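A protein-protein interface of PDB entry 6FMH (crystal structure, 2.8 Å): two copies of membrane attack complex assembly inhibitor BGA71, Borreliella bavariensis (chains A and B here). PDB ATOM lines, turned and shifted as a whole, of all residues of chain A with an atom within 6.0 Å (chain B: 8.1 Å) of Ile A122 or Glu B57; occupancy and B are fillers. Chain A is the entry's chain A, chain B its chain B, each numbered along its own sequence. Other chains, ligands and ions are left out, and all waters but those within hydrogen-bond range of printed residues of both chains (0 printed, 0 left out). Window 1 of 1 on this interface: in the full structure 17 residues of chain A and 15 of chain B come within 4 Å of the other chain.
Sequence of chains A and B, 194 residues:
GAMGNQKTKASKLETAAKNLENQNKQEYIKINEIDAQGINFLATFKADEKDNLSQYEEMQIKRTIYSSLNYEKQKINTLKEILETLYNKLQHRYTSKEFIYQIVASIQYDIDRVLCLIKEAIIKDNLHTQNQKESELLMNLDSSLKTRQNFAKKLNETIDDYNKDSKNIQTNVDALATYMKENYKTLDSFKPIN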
ATOM      1  N   LEU A  13      12.122 -26.868 -37.413  1.00  0.00           N
ATOM      2  CA  LEU A  13      12.512 -27.847 -36.398  1.00  0.00           C
ATOM      3  C   LEU A  13      12.621 -27.187 -35.026  1.00  0.00           C
ATOM      4  O   LEU A  13      12.154 -27.737 -34.007  1.00  0.00           O
ATOM      5  CB  LEU A  13      13.873 -28.421 -36.711  1.00  0.00           C
ATOM      6  CG  LEU A  13      14.019 -29.265 -37.974  1.00  0.00           C
ATOM      7  CD1 LEU A  13      15.463 -29.667 -38.275  1.00  0.00           C
ATOM      8  CD2 LEU A  13      13.190 -30.519 -37.961  1.00  0.00           C
ATOM      9  N   GLU A  14      13.185 -25.979 -35.001  1.00  0.00           N
ATOM     10  CA  GLU A  14      13.214 -25.185 -33.771  1.00  0.00           C
ATOM     11  C   GLU A  14      11.811 -24.881 -33.229  1.00  0.00           C
ATOM     12  O   GLU A  14      11.570 -25.062 -32.023  1.00  0.00           O
ATOM     13  CB  GLU A  14      14.050 -23.943 -33.962  1.00  0.00           C
ATOM     14  CG  GLU A  14      15.552 -24.247 -34.023  1.00  0.00           C
ATOM     15  CD  GLU A  14      16.433 -23.042 -34.369  1.00  0.00           C
ATOM     16  OE1 GLU A  14      15.987 -22.146 -35.121  1.00  0.00           O
ATOM     17  OE2 GLU A  14      17.587 -23.017 -33.895  1.00  0.00           O
ATOM     18  N   ALA A  17      10.244 -28.402 -31.974  1.00  0.00           N
ATOM     19  CA  ALA A  17      10.719 -28.688 -30.619  1.00  0.00           C
ATOM     20  C   ALA A  17      10.071 -27.763 -29.544  1.00  0.00           C
ATOM     21  O   ALA A  17       9.761 -28.218 -28.452  1.00  0.00           O
ATOM     22  CB  ALA A  17      12.251 -28.621 -30.536  1.00  0.00           C
ATOM     23  N   LEU A 117      15.286 -36.812 -31.585  1.00  0.00           N
ATOM     24  CA  LEU A 117      16.025 -36.737 -32.846  1.00  0.00           C
ATOM     25  C   LEU A 117      15.984 -35.430 -33.588  1.00  0.00           C
ATOM     26  O   LEU A 117      16.836 -35.143 -34.346  1.00  0.00           O
ATOM     27  CB  LEU A 117      15.450 -37.741 -33.820  1.00  0.00           C
ATOM     28  CG  LEU A 117      15.823 -39.190 -33.795  1.00  0.00           C
ATOM     29  CD1 LEU A 117      14.928 -39.975 -34.694  1.00  0.00           C
ATOM     30  CD2 LEU A 117      17.249 -39.341 -34.185  1.00  0.00           C
ATOM     31  N   ILE A 118      14.930 -34.685 -33.398  1.00  0.00           N
ATOM     32  CA  ILE A 118      14.793 -33.333 -33.822  1.00  0.00           C
ATOM     33  C   ILE A 118      15.683 -32.451 -32.991  1.00  0.00           C
ATOM     34  O   ILE A 118      16.170 -31.476 -33.468  1.00  0.00           O
ATOM     35  CB  ILE A 118      13.335 -32.886 -33.647  1.00  0.00           C
ATOM     36  CG1 ILE A 118      12.455 -33.637 -34.618  1.00  0.00           C
ATOM     37  CG2 ILE A 118      13.164 -31.388 -33.801  1.00  0.00           C
ATOM     38  CD1 ILE A 118      11.104 -33.036 -34.883  1.00  0.00           C
ATOM     39  N   LYS A 119      15.859 -32.781 -31.733  1.00  0.00           N
ATOM     40  CA  LYS A 119      16.762 -32.056 -30.901  1.00  0.00           C
ATOM     41  C   LYS A 119      18.188 -32.232 -31.356  1.00  0.00           C
ATOM     42  O   LYS A 119      18.933 -31.304 -31.344  1.00  0.00           O
ATOM     43  CB  LYS A 119      16.565 -32.444 -29.451  1.00  0.00           C
ATOM     44  CG  LYS A 119      15.403 -31.762 -28.775  1.00  0.00           C
ATOM     45  CD  LYS A 119      15.127 -32.401 -27.465  1.00  0.00           C
ATOM     46  CE  LYS A 119      14.120 -31.641 -26.666  1.00  0.00           C
ATOM     47  NZ  LYS A 119      13.930 -32.247 -25.349  1.00  0.00           N
ATOM     48  N   GLU A 120      18.558 -33.426 -31.781  1.00  0.00           N
ATOM     49  CA  GLU A 120      19.852 -33.730 -32.362  1.00  0.00           C
ATOM     50  C   GLU A 120      20.210 -32.977 -33.594  1.00  0.00           C
ATOM     51  O   GLU A 120      21.323 -32.691 -33.805  1.00  0.00           O
ATOM     52  CB  GLU A 120      19.916 -35.196 -32.720  1.00  0.00           C
ATOM     53  CG  GLU A 120      21.211 -35.639 -33.381  1.00  0.00           C
ATOM     54  CD  GLU A 120      21.115 -36.983 -33.972  1.00  0.00           C
ATOM     55  OE1 GLU A 120      20.103 -37.266 -34.499  1.00  0.00           O
ATOM     56  OE2 GLU A 120      22.040 -37.750 -33.899  1.00  0.00           O
ATOM     57  N   ALA A 121      19.266 -32.742 -34.463  1.00  0.00           N
ATOM     58  CA  ALA A 121      19.479 -31.947 -35.632  1.00  0.00           C
ATOM     59  C   ALA A 121      19.620 -30.493 -35.294  1.00  0.00           C
ATOM     60  O   ALA A 121      20.400 -29.833 -35.858  1.00  0.00           O
ATOM     61  CB  ALA A 121      18.357 -32.150 -36.600  1.00  0.00           C
ATOM     62  N   ILE A 122      18.845 -29.994 -34.365  1.00  0.00           N
ATOM     63  CA  ILE A 122      19.004 -28.616 -33.961  1.00  0.00           C
ATOM     64  C   ILE A 122      20.421 -28.335 -33.408  1.00  0.00           C
ATOM     65  O   ILE A 122      21.123 -27.432 -33.891  1.00  0.00           O
ATOM     66  CB  ILE A 122      17.988 -28.265 -32.896  1.00  0.00           C
ATOM     67  CG1 ILE A 122      16.594 -28.217 -33.502  1.00  0.00           C
ATOM     68  CG2 ILE A 122      18.277 -26.906 -32.288  1.00  0.00           C
ATOM     69  CD1 ILE A 122      15.506 -27.978 -32.471  1.00  0.00           C
ATOM     70  N   ILE A 123      20.873 -29.189 -32.493  1.00  0.00           N
ATOM     71  CA  ILE A 123      22.112 -28.976 -31.747  1.00  0.00           C
ATOM     72  C   ILE A 123      23.382 -29.443 -32.447  1.00  0.00           C
ATOM     73  O   ILE A 123      24.259 -28.670 -32.742  1.00  0.00           O
ATOM     74  CB  ILE A 123      22.066 -29.640 -30.352  1.00  0.00           C
ATOM     75  CG1 ILE A 123      20.989 -29.008 -29.499  1.00  0.00           C
ATOM     76  CG2 ILE A 123      23.391 -29.464 -29.624  1.00  0.00           C
ATOM     77  CD1 ILE A 123      20.724 -29.734 -28.207  1.00  0.00           C
ATOM     78  N   LYS A 124      23.480 -30.722 -32.711  1.00  0.00           N
ATOM     79  CA  LYS A 124      24.705 -31.303 -33.285  1.00  0.00           C
ATOM     80  C   LYS A 124      24.960 -31.048 -34.773  1.00  0.00           C
ATOM     81  O   LYS A 124      26.118 -31.049 -35.193  1.00  0.00           O
ATOM     82  CB  LYS A 124      24.737 -32.810 -33.024  1.00  0.00           C
ATOM     83  CG  LYS A 124      25.356 -33.109 -31.676  1.00  0.00           C
ATOM     84  CD  LYS A 124      26.857 -33.193 -31.822  1.00  0.00           C
ATOM     85  CE  LYS A 124      27.551 -33.065 -30.487  1.00  0.00           C
ATOM     86  NZ  LYS A 124      29.027 -32.924 -30.645  1.00  0.00           N
ATOM     87  N   ASP A 125      23.917 -30.818 -35.557  1.00  0.00           N
ATOM     88  CA  ASP A 125      24.057 -30.735 -36.980  1.00  0.00           C
ATOM     89  C   ASP A 125      24.019 -29.329 -37.519  1.00  0.00           C
ATOM     90  O   ASP A 125      23.369 -28.451 -37.011  1.00  0.00           O
ATOM     91  CB  ASP A 125      22.987 -31.584 -37.664  1.00  0.00           C
ATOM     92  CG  ASP A 125      23.047 -33.049 -37.246  1.00  0.00           C
ATOM     93  OD1 ASP A 125      23.924 -33.385 -36.426  1.00  0.00           O
ATOM     94  OD2 ASP A 125      22.250 -33.859 -37.747  1.00  0.00           O
ATOM     95  N   GLN A 130      20.861 -30.466 -41.424  1.00  0.00           N
ATOM     96  CA  GLN A 130      19.611 -30.057 -40.803  1.00  0.00           C
ATOM     97  C   GLN A 130      18.494 -29.957 -41.766  1.00  0.00           C
ATOM     98  O   GLN A 130      17.381 -30.365 -41.459  1.00  0.00           O
ATOM     99  CB  GLN A 130      19.758 -28.698 -40.184  1.00  0.00           C
ATOM    100  CG  GLN A 130      18.729 -28.433 -39.109  1.00  0.00           C
ATOM    101  CD  GLN A 130      19.181 -27.310 -38.233  1.00  0.00           C
ATOM    102  OE1 GLN A 130      20.228 -27.391 -37.558  1.00  0.00           O
ATOM    103  NE2 GLN A 130      18.415 -26.241 -38.244  1.00  0.00           N
ATOM    104  N   LEU B  42      22.509 -15.115 -21.239  1.00  0.00           N
ATOM    105  CA  LEU B  42      22.898 -15.219 -22.637  1.00  0.00           C
ATOM    106  C   LEU B  42      22.295 -14.128 -23.513  1.00  0.00           C
ATOM    107  O   LEU B  42      22.173 -14.300 -24.708  1.00  0.00           O
ATOM    108  CB  LEU B  42      22.530 -16.590 -23.182  1.00  0.00           C
ATOM    109  CG  LEU B  42      23.231 -17.803 -22.554  1.00  0.00           C
ATOM    110  CD1 LEU B  42      22.561 -19.103 -22.966  1.00  0.00           C
ATOM    111  CD2 LEU B  42      24.707 -17.883 -22.910  1.00  0.00           C
ATOM    112  N   ASP B  51      23.448 -16.473 -35.664  1.00  0.00           N
ATOM    113  CA  ASP B  51      23.054 -17.718 -35.023  1.00  0.00           C
ATOM    114  C   ASP B  51      21.830 -17.562 -34.218  1.00  0.00           C
ATOM    115  O   ASP B  51      21.440 -16.471 -33.882  1.00  0.00           O
ATOM    116  CB  ASP B  51      24.134 -18.225 -34.103  1.00  0.00           C
ATOM    117  CG  ASP B  51      25.352 -18.597 -34.842  1.00  0.00           C
ATOM    118  OD1 ASP B  51      25.620 -17.948 -35.845  1.00  0.00           O
ATOM    119  OD2 ASP B  51      26.023 -19.553 -34.463  1.00  0.00           O
ATOM    120  N   ASN B  52      21.226 -18.694 -33.918  1.00  0.00           N
ATOM    121  CA  ASN B  52      20.007 -18.721 -33.136  1.00  0.00           C
ATOM    122  C   ASN B  52      20.059 -19.628 -31.960  1.00  0.00           C
ATOM    123  O   ASN B  52      20.343 -20.795 -32.063  1.00  0.00           O
ATOM    124  CB  ASN B  52      18.812 -19.114 -33.971  1.00  0.00           C
ATOM    125  CG  ASN B  52      17.501 -18.826 -33.302  1.00  0.00           C
ATOM    126  OD1 ASN B  52      16.483 -18.848 -33.934  1.00  0.00           O
ATOM    127  ND2 ASN B  52      17.522 -18.571 -32.036  1.00  0.00           N
ATOM    128  N   LEU B  53      19.774 -19.045 -30.826  1.00  0.00           N
ATOM    129  CA  LEU B  53      19.602 -19.741 -29.600  1.00  0.00           C
ATOM    130  C   LEU B  53      18.127 -19.811 -29.435  1.00  0.00           C
ATOM    131  O   LEU B  53      17.476 -18.814 -29.300  1.00  0.00           O
ATOM    132  CB  LEU B  53      20.186 -18.887 -28.492  1.00  0.00           C
ATOM    133  CG  LEU B  53      20.772 -19.479 -27.245  1.00  0.00           C
ATOM    134  CD1 LEU B  53      21.533 -20.727 -27.576  1.00  0.00           C
ATOM    135  CD2 LEU B  53      21.656 -18.454 -26.625  1.00  0.00           C
ATOM    136  N   SER B  54      17.610 -21.011 -29.470  1.00  0.00           N
ATOM    137  CA  SER B  54      16.262 -21.269 -29.136  1.00  0.00           C
ATOM    138  C   SER B  54      16.235 -21.391 -27.656  1.00  0.00           C
ATOM    139  O   SER B  54      17.254 -21.506 -27.069  1.00  0.00           O
ATOM    140  CB  SER B  54      15.808 -22.517 -29.820  1.00  0.00           C
ATOM    141  OG  SER B  54      16.431 -23.621 -29.329  1.00  0.00           O
ATOM    142  N   GLN B  55      15.072 -21.303 -27.056  1.00  0.00           N
ATOM    143  CA  GLN B  55      14.944 -21.340 -25.629  1.00  0.00           C
ATOM    144  C   GLN B  55      15.257 -22.709 -25.004  1.00  0.00           C
ATOM    145  O   GLN B  55      15.555 -22.789 -23.842  1.00  0.00           O
ATOM    146  CB  GLN B  55      13.590 -20.753 -25.245  1.00  0.00           C
ATOM    147  CG  GLN B  55      12.783 -21.518 -24.243  1.00  0.00           C
ATOM    148  CD  GLN B  55      11.390 -21.035 -24.136  1.00  0.00           C
ATOM    149  OE1 GLN B  55      10.947 -20.273 -24.946  1.00  0.00           O
ATOM    150  NE2 GLN B  55      10.693 -21.476 -23.124  1.00  0.00           N
ATOM    151  N   TYR B  56      15.199 -23.764 -25.807  1.00  0.00           N
ATOM    152  CA  TYR B  56      15.657 -25.083 -25.464  1.00  0.00           C
ATOM    153  C   TYR B  56      17.143 -25.159 -25.439  1.00  0.00           C
ATOM    154  O   TYR B  56      17.728 -25.618 -24.523  1.00  0.00           O
ATOM    155  CB  TYR B  56      15.133 -26.135 -26.439  1.00  0.00           C
ATOM    156  CG  TYR B  56      15.719 -27.506 -26.173  1.00  0.00           C
ATOM    157  CD1 TYR B  56      15.468 -28.151 -25.006  1.00  0.00           C
ATOM    158  CD2 TYR B  56      16.611 -28.059 -27.030  1.00  0.00           C
ATOM    159  CE1 TYR B  56      16.047 -29.319 -24.738  1.00  0.00           C
ATOM    160  CE2 TYR B  56      17.205 -29.224 -26.746  1.00  0.00           C
ATOM    161  CZ  TYR B  56      16.902 -29.848 -25.605  1.00  0.00           C
ATOM    162  OH  TYR B  56      17.480 -31.028 -25.323  1.00  0.00           O
ATOM    163  N   GLU B  57      17.762 -24.756 -26.521  1.00  0.00           N
ATOM    164  CA  GLU B  57      19.185 -24.687 -26.601  1.00  0.00           C
ATOM    165  C   GLU B  57      19.704 -23.913 -25.407  1.00  0.00           C
ATOM    166  O   GLU B  57      20.597 -24.346 -24.760  1.00  0.00           O
ATOM    167  CB  GLU B  57      19.609 -24.034 -27.893  1.00  0.00           C
ATOM    168  CG  GLU B  57      19.269 -24.803 -29.132  1.00  0.00           C
ATOM    169  CD  GLU B  57      19.988 -24.305 -30.346  1.00  0.00           C
ATOM    170  OE1 GLU B  57      19.526 -23.430 -31.052  1.00  0.00           O
ATOM    171  OE2 GLU B  57      21.046 -24.805 -30.616  1.00  0.00           O
ATOM    172  N   GLU B  58      19.107 -22.775 -25.116  1.00  0.00           N
ATOM    173  CA  GLU B  58      19.499 -21.934 -24.006  1.00  0.00           C
ATOM    174  C   GLU B  58      19.405 -22.599 -22.672  1.00  0.00           C
ATOM    175  O   GLU B  58      20.155 -22.356 -21.804  1.00  0.00           O
ATOM    176  CB  GLU B  58      18.640 -20.698 -24.014  1.00  0.00           C
ATOM    177  CG  GLU B  58      18.611 -19.877 -22.747  1.00  0.00           C
ATOM    178  CD  GLU B  58      17.718 -18.726 -22.839  1.00  0.00           C
ATOM    179  OE1 GLU B  58      16.854 -18.701 -23.684  1.00  0.00           O
ATOM    180  OE2 GLU B  58      17.908 -17.808 -22.086  1.00  0.00           O
ATOM    181  N   MET B  59      18.391 -23.380 -22.502  1.00  0.00           N
ATOM    182  CA  MET B  59      18.176 -24.101 -21.249  1.00  0.00           C
ATOM    183  C   MET B  59      19.257 -25.149 -21.086  1.00  0.00           C
ATOM    184  O   MET B  59      19.794 -25.340 -20.008  1.00  0.00           O
ATOM    185  CB  MET B  59      16.825 -24.793 -21.273  1.00  0.00           C
ATOM    186  CG  MET B  59      15.931 -24.551 -20.091  1.00  0.00           C
ATOM    187  SD  MET B  59      16.659 -24.267 -18.492  1.00  0.00           S
ATOM    188  CE  MET B  59      16.947 -25.907 -17.948  1.00  0.00           C
ATOM    189  N   GLN B  60      19.547 -25.853 -22.173  1.00  0.00           N
ATOM    190  CA  GLN B  60      20.524 -26.921 -22.146  1.00  0.00           C
ATOM    191  C   GLN B  60      21.892 -26.332 -21.780  1.00  0.00           C
ATOM    192  O   GLN B  60      22.574 -26.814 -20.874  1.00  0.00           O
ATOM    193  CB  GLN B  60      20.544 -27.652 -23.494  1.00  0.00           C
ATOM    194  CG  GLN B  60      19.321 -28.505 -23.796  1.00  0.00           C
ATOM    195  CD  GLN B  60      18.821 -29.363 -22.615  1.00  0.00           C
ATOM    196  OE1 GLN B  60      17.969 -28.925 -21.844  1.00  0.00           O
ATOM    197  NE2 GLN B  60      19.430 -30.522 -22.412  1.00  0.00           N
ATOM    198  N   ILE B  61      22.267 -25.253 -22.446  1.00  0.00           N
ATOM    199  CA  ILE B  61      23.525 -24.548 -22.103  1.00  0.00           C
ATOM    200  C   ILE B  61      23.582 -24.225 -20.605  1.00  0.00           C
ATOM    201  O   ILE B  61      24.583 -24.563 -19.947  1.00  0.00           O
ATOM    202  CB  ILE B  61      23.726 -23.285 -22.941  1.00  0.00           C
ATOM    203  CG1 ILE B  61      24.009 -23.687 -24.366  1.00  0.00           C
ATOM    204  CG2 ILE B  61      24.871 -22.463 -22.417  1.00  0.00           C
ATOM    205  CD1 ILE B  61      23.710 -22.607 -25.402  1.00  0.00           C
ATOM    206  N   LYS B  62      22.507 -23.629 -20.070  1.00  0.00           N
ATOM    207  CA  LYS B  62      22.394 -23.286 -18.615  1.00  0.00           C
ATOM    208  C   LYS B  62      22.414 -24.457 -17.672  1.00  0.00           C
ATOM    209  O   LYS B  62      23.024 -24.378 -16.585  1.00  0.00           O
ATOM    210  CB  LYS B  62      21.140 -22.519 -18.338  1.00  0.00           C
ATOM    211  CG  LYS B  62      21.169 -21.095 -18.884  1.00  0.00           C
ATOM    212  CD  LYS B  62      19.797 -20.480 -18.728  1.00  0.00           C
ATOM    213  CE  LYS B  62      19.756 -19.043 -19.212  1.00  0.00           C
ATOM    214  NZ  LYS B  62      18.355 -18.597 -19.428  1.00  0.00           N
ATOM    215  N   ARG B  63      21.860 -25.584 -18.101  1.00  0.00           N
ATOM    216  CA  ARG B  63      21.974 -26.799 -17.299  1.00  0.00           C
ATOM    217  C   ARG B  63      23.424 -27.127 -16.969  1.00  0.00           C
ATOM    218  O   ARG B  63      23.750 -27.376 -15.806  1.00  0.00           O
ATOM    219  CB  ARG B  63      21.331 -27.988 -17.979  1.00  0.00           C
ATOM    220  CG  ARG B  63      19.825 -27.876 -18.071  1.00  0.00           C
ATOM    221  CD  ARG B  63      19.279 -28.981 -18.893  1.00  0.00           C
ATOM    222  NE  ARG B  63      17.836 -28.995 -18.896  1.00  0.00           N
ATOM    223  CZ  ARG B  63      17.067 -29.399 -17.911  1.00  0.00           C
ATOM    224  NH1 ARG B  63      17.570 -29.840 -16.805  1.00  0.00           N
ATOM    225  NH2 ARG B  63      15.755 -29.381 -18.068  1.00  0.00           N
ATOM    226  N   ILE B 100      30.315 -21.917 -26.191  1.00  0.00           N
ATOM    227  CA  ILE B 100      28.915 -22.103 -25.941  1.00  0.00           C
ATOM    228  C   ILE B 100      28.362 -23.270 -26.757  1.00  0.00           C
ATOM    229  O   ILE B 100      27.729 -24.179 -26.220  1.00  0.00           O
ATOM    230  CB  ILE B 100      28.157 -20.759 -26.242  1.00  0.00           C
ATOM    231  CG1 ILE B 100      28.223 -19.833 -25.030  1.00  0.00           C
ATOM    232  CG2 ILE B 100      26.691 -20.967 -26.618  1.00  0.00           C
ATOM    233  CD1 ILE B 100      27.870 -20.486 -23.704  1.00  0.00           C
ATOM    234  N   TYR B 101      28.480 -23.163 -28.079  1.00  0.00           N
ATOM    235  CA  TYR B 101      27.772 -24.072 -28.971  1.00  0.00           C
ATOM    236  C   TYR B 101      28.547 -25.336 -29.167  1.00  0.00           C
ATOM    237  O   TYR B 101      27.932 -26.366 -29.342  1.00  0.00           O
ATOM    238  CB  TYR B 101      27.454 -23.408 -30.322  1.00  0.00           C
ATOM    239  CG  TYR B 101      26.502 -22.231 -30.224  1.00  0.00           C
ATOM    240  CD1 TYR B 101      25.206 -22.369 -29.710  1.00  0.00           C
ATOM    241  CD2 TYR B 101      26.879 -20.976 -30.682  1.00  0.00           C
ATOM    242  CE1 TYR B 101      24.331 -21.298 -29.650  1.00  0.00           C
ATOM    243  CE2 TYR B 101      26.021 -19.908 -30.616  1.00  0.00           C
ATOM    244  CZ  TYR B 101      24.760 -20.078 -30.112  1.00  0.00           C
ATOM    245  OH  TYR B 101      23.959 -19.000 -30.050  1.00  0.00           O
ATOM    246  N   VAL B 104      30.034 -26.430 -24.439  1.00  0.00           N
ATOM    247  CA  VAL B 104      29.071 -26.545 -23.377  1.00  0.00           C
ATOM    248  C   VAL B 104      27.885 -27.358 -23.835  1.00  0.00           C
ATOM    249  O   VAL B 104      27.407 -28.241 -23.130  1.00  0.00           O
ATOM    250  CB  VAL B 104      28.636 -25.145 -22.841  1.00  0.00           C
ATOM    251  CG1 VAL B 104      27.482 -25.259 -21.873  1.00  0.00           C
ATOM    252  CG2 VAL B 104      29.816 -24.450 -22.163  1.00  0.00           C
ATOM    253  N   ALA B 105      27.399 -27.046 -25.018  1.00  0.00           N
ATOM    254  CA  ALA B 105      26.201 -27.669 -25.559  1.00  0.00           C
ATOM    255  C   ALA B 105      26.423 -29.158 -25.842  1.00  0.00           C
ATOM    256  O   ALA B 105      25.494 -29.949 -25.773  1.00  0.00           O
ATOM    257  CB  ALA B 105      25.761 -26.945 -26.819  1.00  0.00           C
ATOM    258  N   GLN B 108      26.447 -31.123 -22.564  1.00  0.00           N
ATOM    259  CA  GLN B 108      25.061 -31.345 -22.275  1.00  0.00           C
ATOM    260  C   GLN B 108      24.453 -32.402 -23.214  1.00  0.00           C
ATOM    261  O   GLN B 108      23.775 -33.360 -22.744  1.00  0.00           O
ATOM    262  CB  GLN B 108      24.279 -30.040 -22.392  1.00  0.00           C
ATOM    263  CG  GLN B 108      23.732 -29.507 -21.087  1.00  0.00           C
ATOM    264  CD  GLN B 108      23.062 -30.524 -20.247  1.00  0.00           C
ATOM    265  OE1 GLN B 108      22.281 -31.347 -20.732  1.00  0.00           O
ATOM    266  NE2 GLN B 108      23.319 -30.453 -18.961  1.00  0.00           N
ATOM    267  N   TYR B 109      24.683 -32.272 -24.521  1.00  0.00           N
ATOM    268  CA  TYR B 109      23.958 -33.113 -25.473  1.00  0.00           C
ATOM    269  C   TYR B 109      24.239 -34.591 -25.276  1.00  0.00           C
ATOM    270  O   TYR B 109      23.292 -35.400 -25.228  1.00  0.00           O
ATOM    271  CB  TYR B 109      24.226 -32.784 -26.923  1.00  0.00           C
ATOM    272  CG  TYR B 109      23.554 -33.822 -27.775  1.00  0.00           C
ATOM    273  CD1 TYR B 109      22.141 -33.890 -27.862  1.00  0.00           C
ATOM    274  CD2 TYR B 109      24.283 -34.755 -28.462  1.00  0.00           C
ATOM    275  CE1 TYR B 109      21.483 -34.844 -28.628  1.00  0.00           C
ATOM    276  CE2 TYR B 109      23.652 -35.718 -29.265  1.00  0.00           C
ATOM    277  CZ  TYR B 109      22.249 -35.777 -29.317  1.00  0.00           C
ATOM    278  OH  TYR B 109      21.627 -36.667 -30.120  1.00  0.00           O
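The side-chain carboxylate (OE2) of Glu A14 lies close to the side-chain carboxylate (OE1) of Glu B57.
The side-chain hydroxyl (OG) of Ser B54 lies close to the backbone NH (N) of Glu B57 (3.3 Å).
OD1 of Asn B52 touches OE1 of Glu A14 (3.5 Å).
CD of Lys A119 touches OH of Tyr B56, at 3.5 Å.
Glu A120 touches Tyr B109.
Glu B57 touches Ile A122 (CD to CG2, 3.7 Å).
Ile A123 touches Tyr B56.
CD2 of Tyr B109 touches CG of Lys A124 (3.8 Å).
Of chain B, only Glu B57 comes within 4 Å of Ile A122.
Glu B57 touches two residues of chain A.
Of the printed residues of chain B, Glu A120 touches Tyr B109 (3.4 Å).
Of the printed residues of chain B, Lys A119 touches Tyr B56 (3.5 Å).
Of the printed residues of chain B, Glu A14 touches Asn B52 and Glu B57.
Printed residues of chain A within 4 Å of Tyr B56: Lys A119 (3.5 Å) and Ile A123 (3.8 Å).
Leu A13 touches none of the printed residues of chain B.
The nearest residue of chain A that does not touch Glu B57 is Ile A123 (4.3 Å).
Of the 13 printed residues of chain A, 6 touch a printed residue of chain B.
Hydrophobic or aromatic side chains of chain B within 4 Å of the printed part of chain A: Tyr B56 and Tyr B109.
Among the printed residues, no Asp or Glu carboxylate lies within 4 Å of a Lys or Arg side-chain nitrogen of the other chain.
No position is printed for both chains.
Of the 7 pairs that touch across the chains among the printed residues, none has its exchanged pair printed and touching as well.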
